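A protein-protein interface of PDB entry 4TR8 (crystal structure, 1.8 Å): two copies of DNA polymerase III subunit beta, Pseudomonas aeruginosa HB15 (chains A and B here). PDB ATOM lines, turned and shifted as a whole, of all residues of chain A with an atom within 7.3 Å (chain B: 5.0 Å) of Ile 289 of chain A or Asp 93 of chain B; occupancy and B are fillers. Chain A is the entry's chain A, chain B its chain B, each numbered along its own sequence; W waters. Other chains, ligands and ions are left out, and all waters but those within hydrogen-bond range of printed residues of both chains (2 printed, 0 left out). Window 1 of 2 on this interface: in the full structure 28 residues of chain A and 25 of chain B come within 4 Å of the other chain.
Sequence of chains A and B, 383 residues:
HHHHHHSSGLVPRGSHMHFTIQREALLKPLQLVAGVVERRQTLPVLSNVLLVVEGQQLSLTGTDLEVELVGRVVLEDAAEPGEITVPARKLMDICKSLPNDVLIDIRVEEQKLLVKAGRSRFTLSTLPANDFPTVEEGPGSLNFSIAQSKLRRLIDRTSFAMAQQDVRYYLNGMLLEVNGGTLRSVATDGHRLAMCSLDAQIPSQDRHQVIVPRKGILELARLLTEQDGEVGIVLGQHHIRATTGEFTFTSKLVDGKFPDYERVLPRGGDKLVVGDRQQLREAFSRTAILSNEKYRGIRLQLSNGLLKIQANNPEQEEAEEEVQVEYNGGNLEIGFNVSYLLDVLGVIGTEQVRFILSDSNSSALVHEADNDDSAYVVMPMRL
Printed residues of chain B within 4 Å of Arg 286 of chain A: Ser 97 (2.9 Å). Of the printed residues of chain B, Ile 289 of chain A touches Asp 93 (3.6 Å), Ile 94 (3.8 Å) and Ser 97 (3.7 Å). Of the printed residues of chain B, Asn 313 of chain A touches Lys 90 (3.8 Å). Of the printed residues of chain A, Lys 90 of chain B touches Leu 290 (3.9 Å), Asn 313 (3.8 Å) and Glu 317 (2.7 Å). Of chain A, only Ile 289 comes within 4 Å of Asp 93 of chain B. Of the printed residues of chain A, Ile 94 of chain B touches Ile 289. Of the printed residues of chain A, Ser 97 of chain B touches Arg 286 (2.9 Å) and Ile 289 (3.7 Å). The nearest residue of chain B that does not touch Ile 289 of chain A is Lys 90 of chain B (4.3 Å). The nearest printed residue of chain A that does not touch Ile 94 of chain B is Leu 290 of chain A (4.4 Å).
The backbone carbonyl oxygen (O) of Leu 290 of chain A lies within hydrogen-bond range of the backbone NH (N) of Asn 313 of chain A. The backbone carbonyl oxygen (O) of Ile 94 of chain B is in hydrogen-bond range of the side-chain hydroxyl (OG) of Ser 97 of chain B (2.7 Å). The backbone carbonyl oxygen (O) of Asp 93 of chain B sits at hydrogen-bond distance from the side-chain hydroxyl (OG) of Ser 97 of chain B (3.3 Å). The side-chain amide nitrogen of Asn 313 of chain A is in hydrogen-bond range of the side-chain carboxylate of Glu 317 of chain A (2.9 Å).
Ile 289 of chain A touches Asp 93 of chain B (CD1 to O, 3.6 Å). Ile 94 of chain B touches Ile 289 of chain A (N to CD1, 3.8 Å). Ser 97 of chain B touches Ile 289 of chain A. Lys 90 of chain B touches Leu 290 of chain A (CD to CD2, 3.9 Å). NZ of Lys 90 of chain B touches ND2 of Asn 313 of chain A, 3.8 Å away.
No position is printed for both chains. Of the 7 pairs that touch across the chains among the printed residues, none has its exchanged pair printed and touching as well.
Of the 18 printed residues of chain A, 5 touch a printed residue of chain B. Printed residues of chain B that touch a printed residue of chain A: Lys 90, Asp 93, Ile 94 and Ser 97. Hydrophobic or aromatic side chains of chain B within 4 Å of the printed part of chain A: Ile 94. Among the printed residues, Asp or Glu carboxylates within 4 Å of a Lys or Arg side-chain nitrogen of the other chain: Glu 317 of chain A with Lys 90 of chain B.
The guanidinium group (NH1) of Arg 286 of chain A is in hydrogen-bond range of the backbone carbonyl oxygen (O) of Ser 97 of chain B (2.9 Å). The side-chain amino group of Lys 90 of chain B is in salt-bridge range of the side-chain carboxylate of Glu 317 of chain A (2.7 Å).
Water W2 bridges OE2 of Glu 293 of chain A (2.7 Å) and NZ of Lys 90 of chain B (3.0 Å). Water W1 lies within hydrogen-bond range of the side-chain amino group (NZ) of Lys 90 of chain B (3.0 Å) and the side-chain carboxylate (OE2) of Glu 317 of chain A (3.2 Å).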
ATOM      1  N   ALA A 283      -9.376 -21.637  -4.875  1.00  0.00           N
ATOM      2  CA  ALA A 283      -8.992 -20.311  -4.361  1.00  0.00           C
ATOM      3  C   ALA A 283      -7.541 -19.990  -4.762  1.00  0.00           C
ATOM      4  O   ALA A 283      -7.274 -18.882  -5.219  1.00  0.00           O
ATOM      5  CB  ALA A 283      -9.138 -20.261  -2.840  1.00  0.00           C
ATOM      6  N   PHE A 284      -6.620 -20.970  -4.646  1.00  0.00           N
ATOM      7  CA  PHE A 284      -5.209 -20.788  -5.026  1.00  0.00           C
ATOM      8  C   PHE A 284      -5.119 -20.490  -6.533  1.00  0.00           C
ATOM      9  O   PHE A 284      -4.398 -19.558  -6.917  1.00  0.00           O
ATOM     10  CB  PHE A 284      -4.358 -22.021  -4.670  1.00  0.00           C
ATOM     11  CG  PHE A 284      -4.086 -22.279  -3.202  1.00  0.00           C
ATOM     12  CD1 PHE A 284      -4.090 -21.241  -2.277  1.00  0.00           C
ATOM     13  CD2 PHE A 284      -3.827 -23.565  -2.745  1.00  0.00           C
ATOM     14  CE1 PHE A 284      -3.838 -21.486  -0.919  1.00  0.00           C
ATOM     15  CE2 PHE A 284      -3.556 -23.801  -1.389  1.00  0.00           C
ATOM     16  CZ  PHE A 284      -3.593 -22.769  -0.487  1.00  0.00           C
ATOM     17  N   SER A 285      -5.866 -21.263  -7.356  1.00  0.00           N
ATOM     18  CA  SER A 285      -5.902 -21.087  -8.809  1.00  0.00           C
ATOM     19  C   SER A 285      -6.426 -19.689  -9.201  1.00  0.00           C
ATOM     20  O   SER A 285      -5.806 -19.024 -10.044  1.00  0.00           O
ATOM     21  CB  SER A 285      -6.735 -22.183  -9.466  1.00  0.00           C
ATOM     22  OG  SER A 285      -6.540 -22.181 -10.871  1.00  0.00           O
ATOM     23  N   ARG A 286      -7.529 -19.225  -8.580  1.00  0.00           N
ATOM     24  CA  ARG A 286      -8.133 -17.901  -8.845  1.00  0.00           C
ATOM     25  C   ARG A 286      -7.162 -16.788  -8.518  1.00  0.00           C
ATOM     26  O   ARG A 286      -6.912 -15.922  -9.354  1.00  0.00           O
ATOM     27  CB  ARG A 286      -9.399 -17.691  -7.988  1.00  0.00           C
ATOM     28  CG  ARG A 286     -10.623 -18.251  -8.626  1.00  0.00           C
ATOM     29  CD  ARG A 286     -11.888 -17.692  -8.012  1.00  0.00           C
ATOM     30  NE  ARG A 286     -12.076 -18.234  -6.677  1.00  0.00           N
ATOM     31  CZ  ARG A 286     -12.668 -19.390  -6.405  1.00  0.00           C
ATOM     32  NH1 ARG A 286     -13.196 -20.122  -7.382  1.00  0.00           N
ATOM     33  NH2 ARG A 286     -12.781 -19.799  -5.159  1.00  0.00           N
ATOM     34  N   THR A 287      -6.617 -16.805  -7.295  1.00  0.00           N
ATOM     35  CA  THR A 287      -5.687 -15.768  -6.851  1.00  0.00           C
ATOM     36  C   THR A 287      -4.400 -15.754  -7.685  1.00  0.00           C
ATOM     37  O   THR A 287      -3.892 -14.666  -7.981  1.00  0.00           O
ATOM     38  CB  THR A 287      -5.436 -15.854  -5.330  1.00  0.00           C
ATOM     39  OG1 THR A 287      -4.744 -17.082  -5.041  1.00  0.00           O
ATOM     40  CG2 THR A 287      -6.737 -15.729  -4.500  1.00  0.00           C
ATOM     41  N   ALA A 288      -3.924 -16.944  -8.126  1.00  0.00           N
ATOM     42  CA  ALA A 288      -2.731 -17.135  -8.969  1.00  0.00           C
ATOM     43  C   ALA A 288      -2.795 -16.341 -10.295  1.00  0.00           C
ATOM     44  O   ALA A 288      -1.750 -16.051 -10.869  1.00  0.00           O
ATOM     45  CB  ALA A 288      -2.537 -18.602  -9.288  1.00  0.00           C
ATOM     46  N   ILE A 289      -4.008 -16.025 -10.786  1.00  0.00           N
ATOM     47  CA  ILE A 289      -4.203 -15.279 -12.047  1.00  0.00           C
ATOM     48  C   ILE A 289      -3.494 -13.915 -11.952  1.00  0.00           C
ATOM     49  O   ILE A 289      -2.985 -13.403 -12.958  1.00  0.00           O
ATOM     50  CB  ILE A 289      -5.716 -15.111 -12.379  1.00  0.00           C
ATOM     51  CG1 ILE A 289      -6.402 -16.480 -12.662  1.00  0.00           C
ATOM     52  CG2 ILE A 289      -5.939 -14.126 -13.570  1.00  0.00           C
ATOM     53  CD1 ILE A 289      -7.984 -16.370 -12.621  1.00  0.00           C
ATOM     54  N   LEU A 290      -3.471 -13.339 -10.743  1.00  0.00           N
ATOM     55  CA  LEU A 290      -2.821 -12.048 -10.516  1.00  0.00           C
ATOM     56  C   LEU A 290      -1.476 -12.148  -9.788  1.00  0.00           C
ATOM     57  O   LEU A 290      -0.981 -11.148  -9.261  1.00  0.00           O
ATOM     58  CB  LEU A 290      -3.796 -11.024  -9.924  1.00  0.00           C
ATOM     59  CG  LEU A 290      -5.071 -10.773 -10.769  1.00  0.00           C
ATOM     60  CD1 LEU A 290      -5.946  -9.731 -10.126  1.00  0.00           C
ATOM     61  CD2 LEU A 290      -4.743 -10.362 -12.232  1.00  0.00           C
ATOM     62  N   SER A 291      -0.875 -13.358  -9.779  1.00  0.00           N
ATOM     63  CA  SER A 291       0.447 -13.559  -9.197  1.00  0.00           C
ATOM     64  C   SER A 291       1.495 -13.255 -10.291  1.00  0.00           C
ATOM     65  O   SER A 291       1.140 -13.149 -11.473  1.00  0.00           O
ATOM     66  CB  SER A 291       0.611 -14.982  -8.668  1.00  0.00           C
ATOM     67  OG  SER A 291       0.762 -15.915  -9.723  1.00  0.00           O
ATOM     68  N   ASN A 292       2.774 -13.120  -9.892  1.00  0.00           N
ATOM     69  CA  ASN A 292       3.907 -12.901 -10.797  1.00  0.00           C
ATOM     70  C   ASN A 292       4.018 -14.132 -11.730  1.00  0.00           C
ATOM     71  O   ASN A 292       4.022 -15.270 -11.255  1.00  0.00           O
ATOM     72  CB  ASN A 292       5.186 -12.718  -9.972  1.00  0.00           C
ATOM     73  CG  ASN A 292       6.403 -12.347 -10.776  1.00  0.00           C
ATOM     74  OD1 ASN A 292       6.941 -13.150 -11.549  1.00  0.00           O
ATOM     75  ND2 ASN A 292       6.895 -11.136 -10.564  1.00  0.00           N
ATOM     76  N   GLU A 293       4.079 -13.893 -13.048  1.00  0.00           N
ATOM     77  CA  GLU A 293       4.140 -14.938 -14.080  1.00  0.00           C
ATOM     78  C   GLU A 293       5.319 -15.922 -13.981  1.00  0.00           C
ATOM     79  O   GLU A 293       5.177 -17.073 -14.401  1.00  0.00           O
ATOM     80  CB  GLU A 293       4.029 -14.323 -15.483  1.00  0.00           C
ATOM     81  CG  GLU A 293       2.647 -13.758 -15.783  1.00  0.00           C
ATOM     82  CD  GLU A 293       2.462 -13.029 -17.102  1.00  0.00           C
ATOM     83  OE1 GLU A 293       3.297 -13.206 -18.019  1.00  0.00           O
ATOM     84  OE2 GLU A 293       1.458 -12.291 -17.223  1.00  0.00           O
ATOM     85  N   ARG A 296       5.375 -16.894  -9.331  1.00  0.00           N
ATOM     86  CA  ARG A 296       4.054 -17.432  -8.931  1.00  0.00           C
ATOM     87  C   ARG A 296       3.784 -17.392  -7.414  1.00  0.00           C
ATOM     88  O   ARG A 296       3.100 -18.264  -6.864  1.00  0.00           O
ATOM     89  CB  ARG A 296       3.851 -18.855  -9.510  1.00  0.00           C
ATOM     90  CG  ARG A 296       3.998 -18.916 -11.033  1.00  0.00           C
ATOM     91  CD  ARG A 296       2.691 -18.656 -11.739  1.00  0.00           C
ATOM     92  NE  ARG A 296       1.769 -19.776 -11.552  1.00  0.00           N
ATOM     93  CZ  ARG A 296       0.457 -19.704 -11.748  1.00  0.00           C
ATOM     94  NH1 ARG A 296      -0.102 -18.564 -12.134  1.00  0.00           N
ATOM     95  NH2 ARG A 296      -0.307 -20.773 -11.555  1.00  0.00           N
ATOM     96  N   ILE A 298       2.328 -16.507  -3.826  1.00  0.00           N
ATOM     97  CA  ILE A 298       1.073 -16.186  -3.147  1.00  0.00           C
ATOM     98  C   ILE A 298       1.318 -16.086  -1.650  1.00  0.00           C
ATOM     99  O   ILE A 298       2.101 -16.849  -1.088  1.00  0.00           O
ATOM    100  CB  ILE A 298      -0.157 -17.045  -3.511  1.00  0.00           C
ATOM    101  CG1 ILE A 298       0.008 -18.517  -3.087  1.00  0.00           C
ATOM    102  CG2 ILE A 298      -0.561 -16.860  -4.988  1.00  0.00           C
ATOM    103  CD1 ILE A 298      -1.302 -19.236  -2.865  1.00  0.00           C
ATOM    104  N   ALA A 311      -2.434 -12.346  -3.784  1.00  0.00           N
ATOM    105  CA  ALA A 311      -1.473 -12.364  -4.881  1.00  0.00           C
ATOM    106  C   ALA A 311      -1.373 -10.973  -5.464  1.00  0.00           C
ATOM    107  O   ALA A 311      -2.373 -10.266  -5.517  1.00  0.00           O
ATOM    108  CB  ALA A 311      -1.875 -13.370  -5.952  1.00  0.00           C
ATOM    109  N   ASN A 313       1.162  -8.730  -8.625  1.00  0.00           N
ATOM    110  CA  ASN A 313       2.074  -8.861  -9.765  1.00  0.00           C
ATOM    111  C   ASN A 313       2.823  -7.514  -9.989  1.00  0.00           C
ATOM    112  O   ASN A 313       2.436  -6.517  -9.361  1.00  0.00           O
ATOM    113  CB  ASN A 313       1.306  -9.331 -11.023  1.00  0.00           C
ATOM    114  CG  ASN A 313       0.207  -8.420 -11.520  1.00  0.00           C
ATOM    115  OD1 ASN A 313       0.167  -7.217 -11.250  1.00  0.00           O
ATOM    116  ND2 ASN A 313      -0.689  -8.978 -12.319  1.00  0.00           N
ATOM    117  N   GLU A 317      -1.536  -5.199  -9.793  1.00  0.00           N
ATOM    118  CA  GLU A 317      -2.843  -5.854  -9.733  1.00  0.00           C
ATOM    119  C   GLU A 317      -2.833  -6.761  -8.499  1.00  0.00           C
ATOM    120  O   GLU A 317      -1.761  -7.178  -8.061  1.00  0.00           O
ATOM    121  CB  GLU A 317      -3.138  -6.646 -11.013  1.00  0.00           C
ATOM    122  CG  GLU A 317      -3.273  -5.741 -12.229  1.00  0.00           C
ATOM    123  CD  GLU A 317      -3.391  -6.455 -13.561  1.00  0.00           C
ATOM    124  OE1 GLU A 317      -2.730  -7.503 -13.740  1.00  0.00           O
ATOM    125  OE2 GLU A 317      -4.114  -5.939 -14.443  1.00  0.00           O
ATOM    126  N   ALA A 319      -5.187  -9.913  -6.127  1.00  0.00           N
ATOM    127  CA  ALA A 319      -6.286 -10.852  -5.941  1.00  0.00           C
ATOM    128  C   ALA A 319      -6.267 -11.283  -4.479  1.00  0.00           C
ATOM    129  O   ALA A 319      -5.195 -11.468  -3.900  1.00  0.00           O
ATOM    130  CB  ALA A 319      -6.137 -12.056  -6.848  1.00  0.00           C
ATOM    131  N   VAL A 338       2.586 -20.803  -5.919  1.00  0.00           N
ATOM    132  CA  VAL A 338       1.240 -21.355  -6.074  1.00  0.00           C
ATOM    133  C   VAL A 338       1.205 -22.645  -6.895  1.00  0.00           C
ATOM    134  O   VAL A 338       0.413 -23.521  -6.563  1.00  0.00           O
ATOM    135  CB  VAL A 338       0.183 -20.305  -6.518  1.00  0.00           C
ATOM    136  CG1 VAL A 338       0.413 -19.866  -7.957  1.00  0.00           C
ATOM    137  CG2 VAL A 338      -1.247 -20.831  -6.328  1.00  0.00           C
ATOM    138  N   ALA B  88      -8.525  -8.264 -21.282  1.00  0.00           N
ATOM    139  CA  ALA B  88      -9.567  -9.199 -21.691  1.00  0.00           C
ATOM    140  C   ALA B  88      -9.325 -10.614 -21.194  1.00  0.00           C
ATOM    141  O   ALA B  88     -10.245 -11.213 -20.627  1.00  0.00           O
ATOM    142  CB  ALA B  88      -9.709  -9.192 -23.205  1.00  0.00           C
ATOM    143  N   ARG B  89      -8.110 -11.154 -21.421  1.00  0.00           N
ATOM    144  CA  ARG B  89      -7.766 -12.525 -20.988  1.00  0.00           C
ATOM    145  C   ARG B  89      -7.870 -12.684 -19.467  1.00  0.00           C
ATOM    146  O   ARG B  89      -8.475 -13.657 -18.996  1.00  0.00           O
ATOM    147  CB  ARG B  89      -6.387 -12.962 -21.545  1.00  0.00           C
ATOM    148  CG  ARG B  89      -5.941 -14.390 -21.174  1.00  0.00           C
ATOM    149  CD  ARG B  89      -6.910 -15.491 -21.593  1.00  0.00           C
ATOM    150  NE  ARG B  89      -6.211 -16.677 -22.088  1.00  0.00           N
ATOM    151  CZ  ARG B  89      -6.137 -17.027 -23.370  1.00  0.00           C
ATOM    152  NH1 ARG B  89      -6.737 -16.295 -24.303  1.00  0.00           N
ATOM    153  NH2 ARG B  89      -5.473 -18.119 -23.727  1.00  0.00           N
ATOM    154  N   LYS B  90      -7.322 -11.713 -18.701  1.00  0.00           N
ATOM    155  CA  LYS B  90      -7.392 -11.736 -17.232  1.00  0.00           C
ATOM    156  C   LYS B  90      -8.830 -11.686 -16.731  1.00  0.00           C
ATOM    157  O   LYS B  90      -9.186 -12.496 -15.883  1.00  0.00           O
ATOM    158  CB  LYS B  90      -6.549 -10.612 -16.598  1.00  0.00           C
ATOM    159  CG  LYS B  90      -5.068 -10.927 -16.568  1.00  0.00           C
ATOM    160  CD  LYS B  90      -4.253  -9.765 -16.037  1.00  0.00           C
ATOM    161  CE  LYS B  90      -2.797 -10.138 -16.024  1.00  0.00           C
ATOM    162  NZ  LYS B  90      -1.925  -8.944 -15.866  1.00  0.00           N
ATOM    163  N   LEU B  91      -9.670 -10.778 -17.285  1.00  0.00           N
ATOM    164  CA  LEU B  91     -11.076 -10.694 -16.864  1.00  0.00           C
ATOM    165  C   LEU B  91     -11.842 -11.972 -17.221  1.00  0.00           C
ATOM    166  O   LEU B  91     -12.639 -12.448 -16.411  1.00  0.00           O
ATOM    167  CB  LEU B  91     -11.786  -9.445 -17.414  1.00  0.00           C
ATOM    168  CG  LEU B  91     -13.193  -9.168 -16.857  1.00  0.00           C
ATOM    169  CD1 LEU B  91     -13.146  -8.784 -15.351  1.00  0.00           C
ATOM    170  CD2 LEU B  91     -13.916  -8.105 -17.678  1.00  0.00           C
ATOM    171  N   MET B  92     -11.596 -12.526 -18.420  1.00  0.00           N
ATOM    172  CA  MET B  92     -12.253 -13.781 -18.815  1.00  0.00           C
ATOM    173  C   MET B  92     -11.832 -14.907 -17.860  1.00  0.00           C
ATOM    174  O   MET B  92     -12.700 -15.638 -17.367  1.00  0.00           O
ATOM    175  CB  MET B  92     -11.925 -14.160 -20.264  1.00  0.00           C
ATOM    176  CG  MET B  92     -12.541 -15.502 -20.676  1.00  0.00           C
ATOM    177  SD  MET B  92     -11.985 -15.973 -22.321  1.00  0.00           S
ATOM    178  N   ASP B  93     -10.507 -15.047 -17.602  1.00  0.00           N
ATOM    179  CA  ASP B  93     -10.000 -16.099 -16.701  1.00  0.00           C
ATOM    180  C   ASP B  93     -10.565 -15.982 -15.292  1.00  0.00           C
ATOM    181  O   ASP B  93     -10.879 -16.994 -14.690  1.00  0.00           O
ATOM    182  CB  ASP B  93      -8.462 -16.133 -16.659  1.00  0.00           C
ATOM    183  CG  ASP B  93      -7.796 -16.588 -17.952  1.00  0.00           C
ATOM    184  OD1 ASP B  93      -8.502 -17.101 -18.831  1.00  0.00           O
ATOM    185  OD2 ASP B  93      -6.564 -16.423 -18.073  1.00  0.00           O
ATOM    186  N   ILE B  94     -10.724 -14.754 -14.787  1.00  0.00           N
ATOM    187  CA  ILE B  94     -11.288 -14.506 -13.462  1.00  0.00           C
ATOM    188  C   ILE B  94     -12.747 -14.968 -13.438  1.00  0.00           C
ATOM    189  O   ILE B  94     -13.122 -15.756 -12.571  1.00  0.00           O
ATOM    190  CB  ILE B  94     -11.104 -13.022 -13.026  1.00  0.00           C
ATOM    191  CG1 ILE B  94      -9.610 -12.753 -12.711  1.00  0.00           C
ATOM    192  CG2 ILE B  94     -11.995 -12.710 -11.787  1.00  0.00           C
ATOM    193  CD1 ILE B  94      -9.224 -11.284 -12.570  1.00  0.00           C
ATOM    194  N   CYS B  95     -13.541 -14.516 -14.414  1.00  0.00           N
ATOM    195  CA  CYS B  95     -14.954 -14.866 -14.529  1.00  0.00           C
ATOM    196  C   CYS B  95     -15.123 -16.401 -14.622  1.00  0.00           C
ATOM    197  O   CYS B  95     -15.928 -16.982 -13.887  1.00  0.00           O
ATOM    198  CB  CYS B  95     -15.576 -14.165 -15.733  1.00  0.00           C
ATOM    199  SG  CYS B  95     -17.372 -14.358 -15.845  1.00  0.00           S
ATOM    200  N   LYS B  96     -14.337 -17.040 -15.503  1.00  0.00           N
ATOM    201  CA  LYS B  96     -14.350 -18.498 -15.708  1.00  0.00           C
ATOM    202  C   LYS B  96     -14.052 -19.253 -14.391  1.00  0.00           C
ATOM    203  O   LYS B  96     -14.697 -20.265 -14.097  1.00  0.00           O
ATOM    204  CB  LYS B  96     -13.289 -18.864 -16.748  1.00  0.00           C
ATOM    205  CG  LYS B  96     -13.519 -20.199 -17.453  1.00  0.00           C
ATOM    206  CD  LYS B  96     -13.548 -20.023 -18.983  1.00  0.00           C
ATOM    207  CE  LYS B  96     -12.196 -19.794 -19.640  1.00  0.00           C
ATOM    208  NZ  LYS B  96     -12.299 -19.752 -21.128  1.00  0.00           N
ATOM    209  N   SER B  97     -13.054 -18.773 -13.632  1.00  0.00           N
ATOM    210  CA  SER B  97     -12.603 -19.401 -12.388  1.00  0.00           C
ATOM    211  C   SER B  97     -13.579 -19.255 -11.226  1.00  0.00           C
ATOM    212  O   SER B  97     -13.446 -19.981 -10.231  1.00  0.00           O
ATOM    213  CB  SER B  97     -11.239 -18.842 -11.989  1.00  0.00           C
ATOM    214  OG  SER B  97     -11.330 -17.516 -11.485  1.00  0.00           O
HETATM  215  O   HOH W   1      -2.324  -6.262 -17.122  1.00  0.00           O
HETATM  216  O   HOH W   2       0.475 -10.703 -15.235  1.00  0.00           O
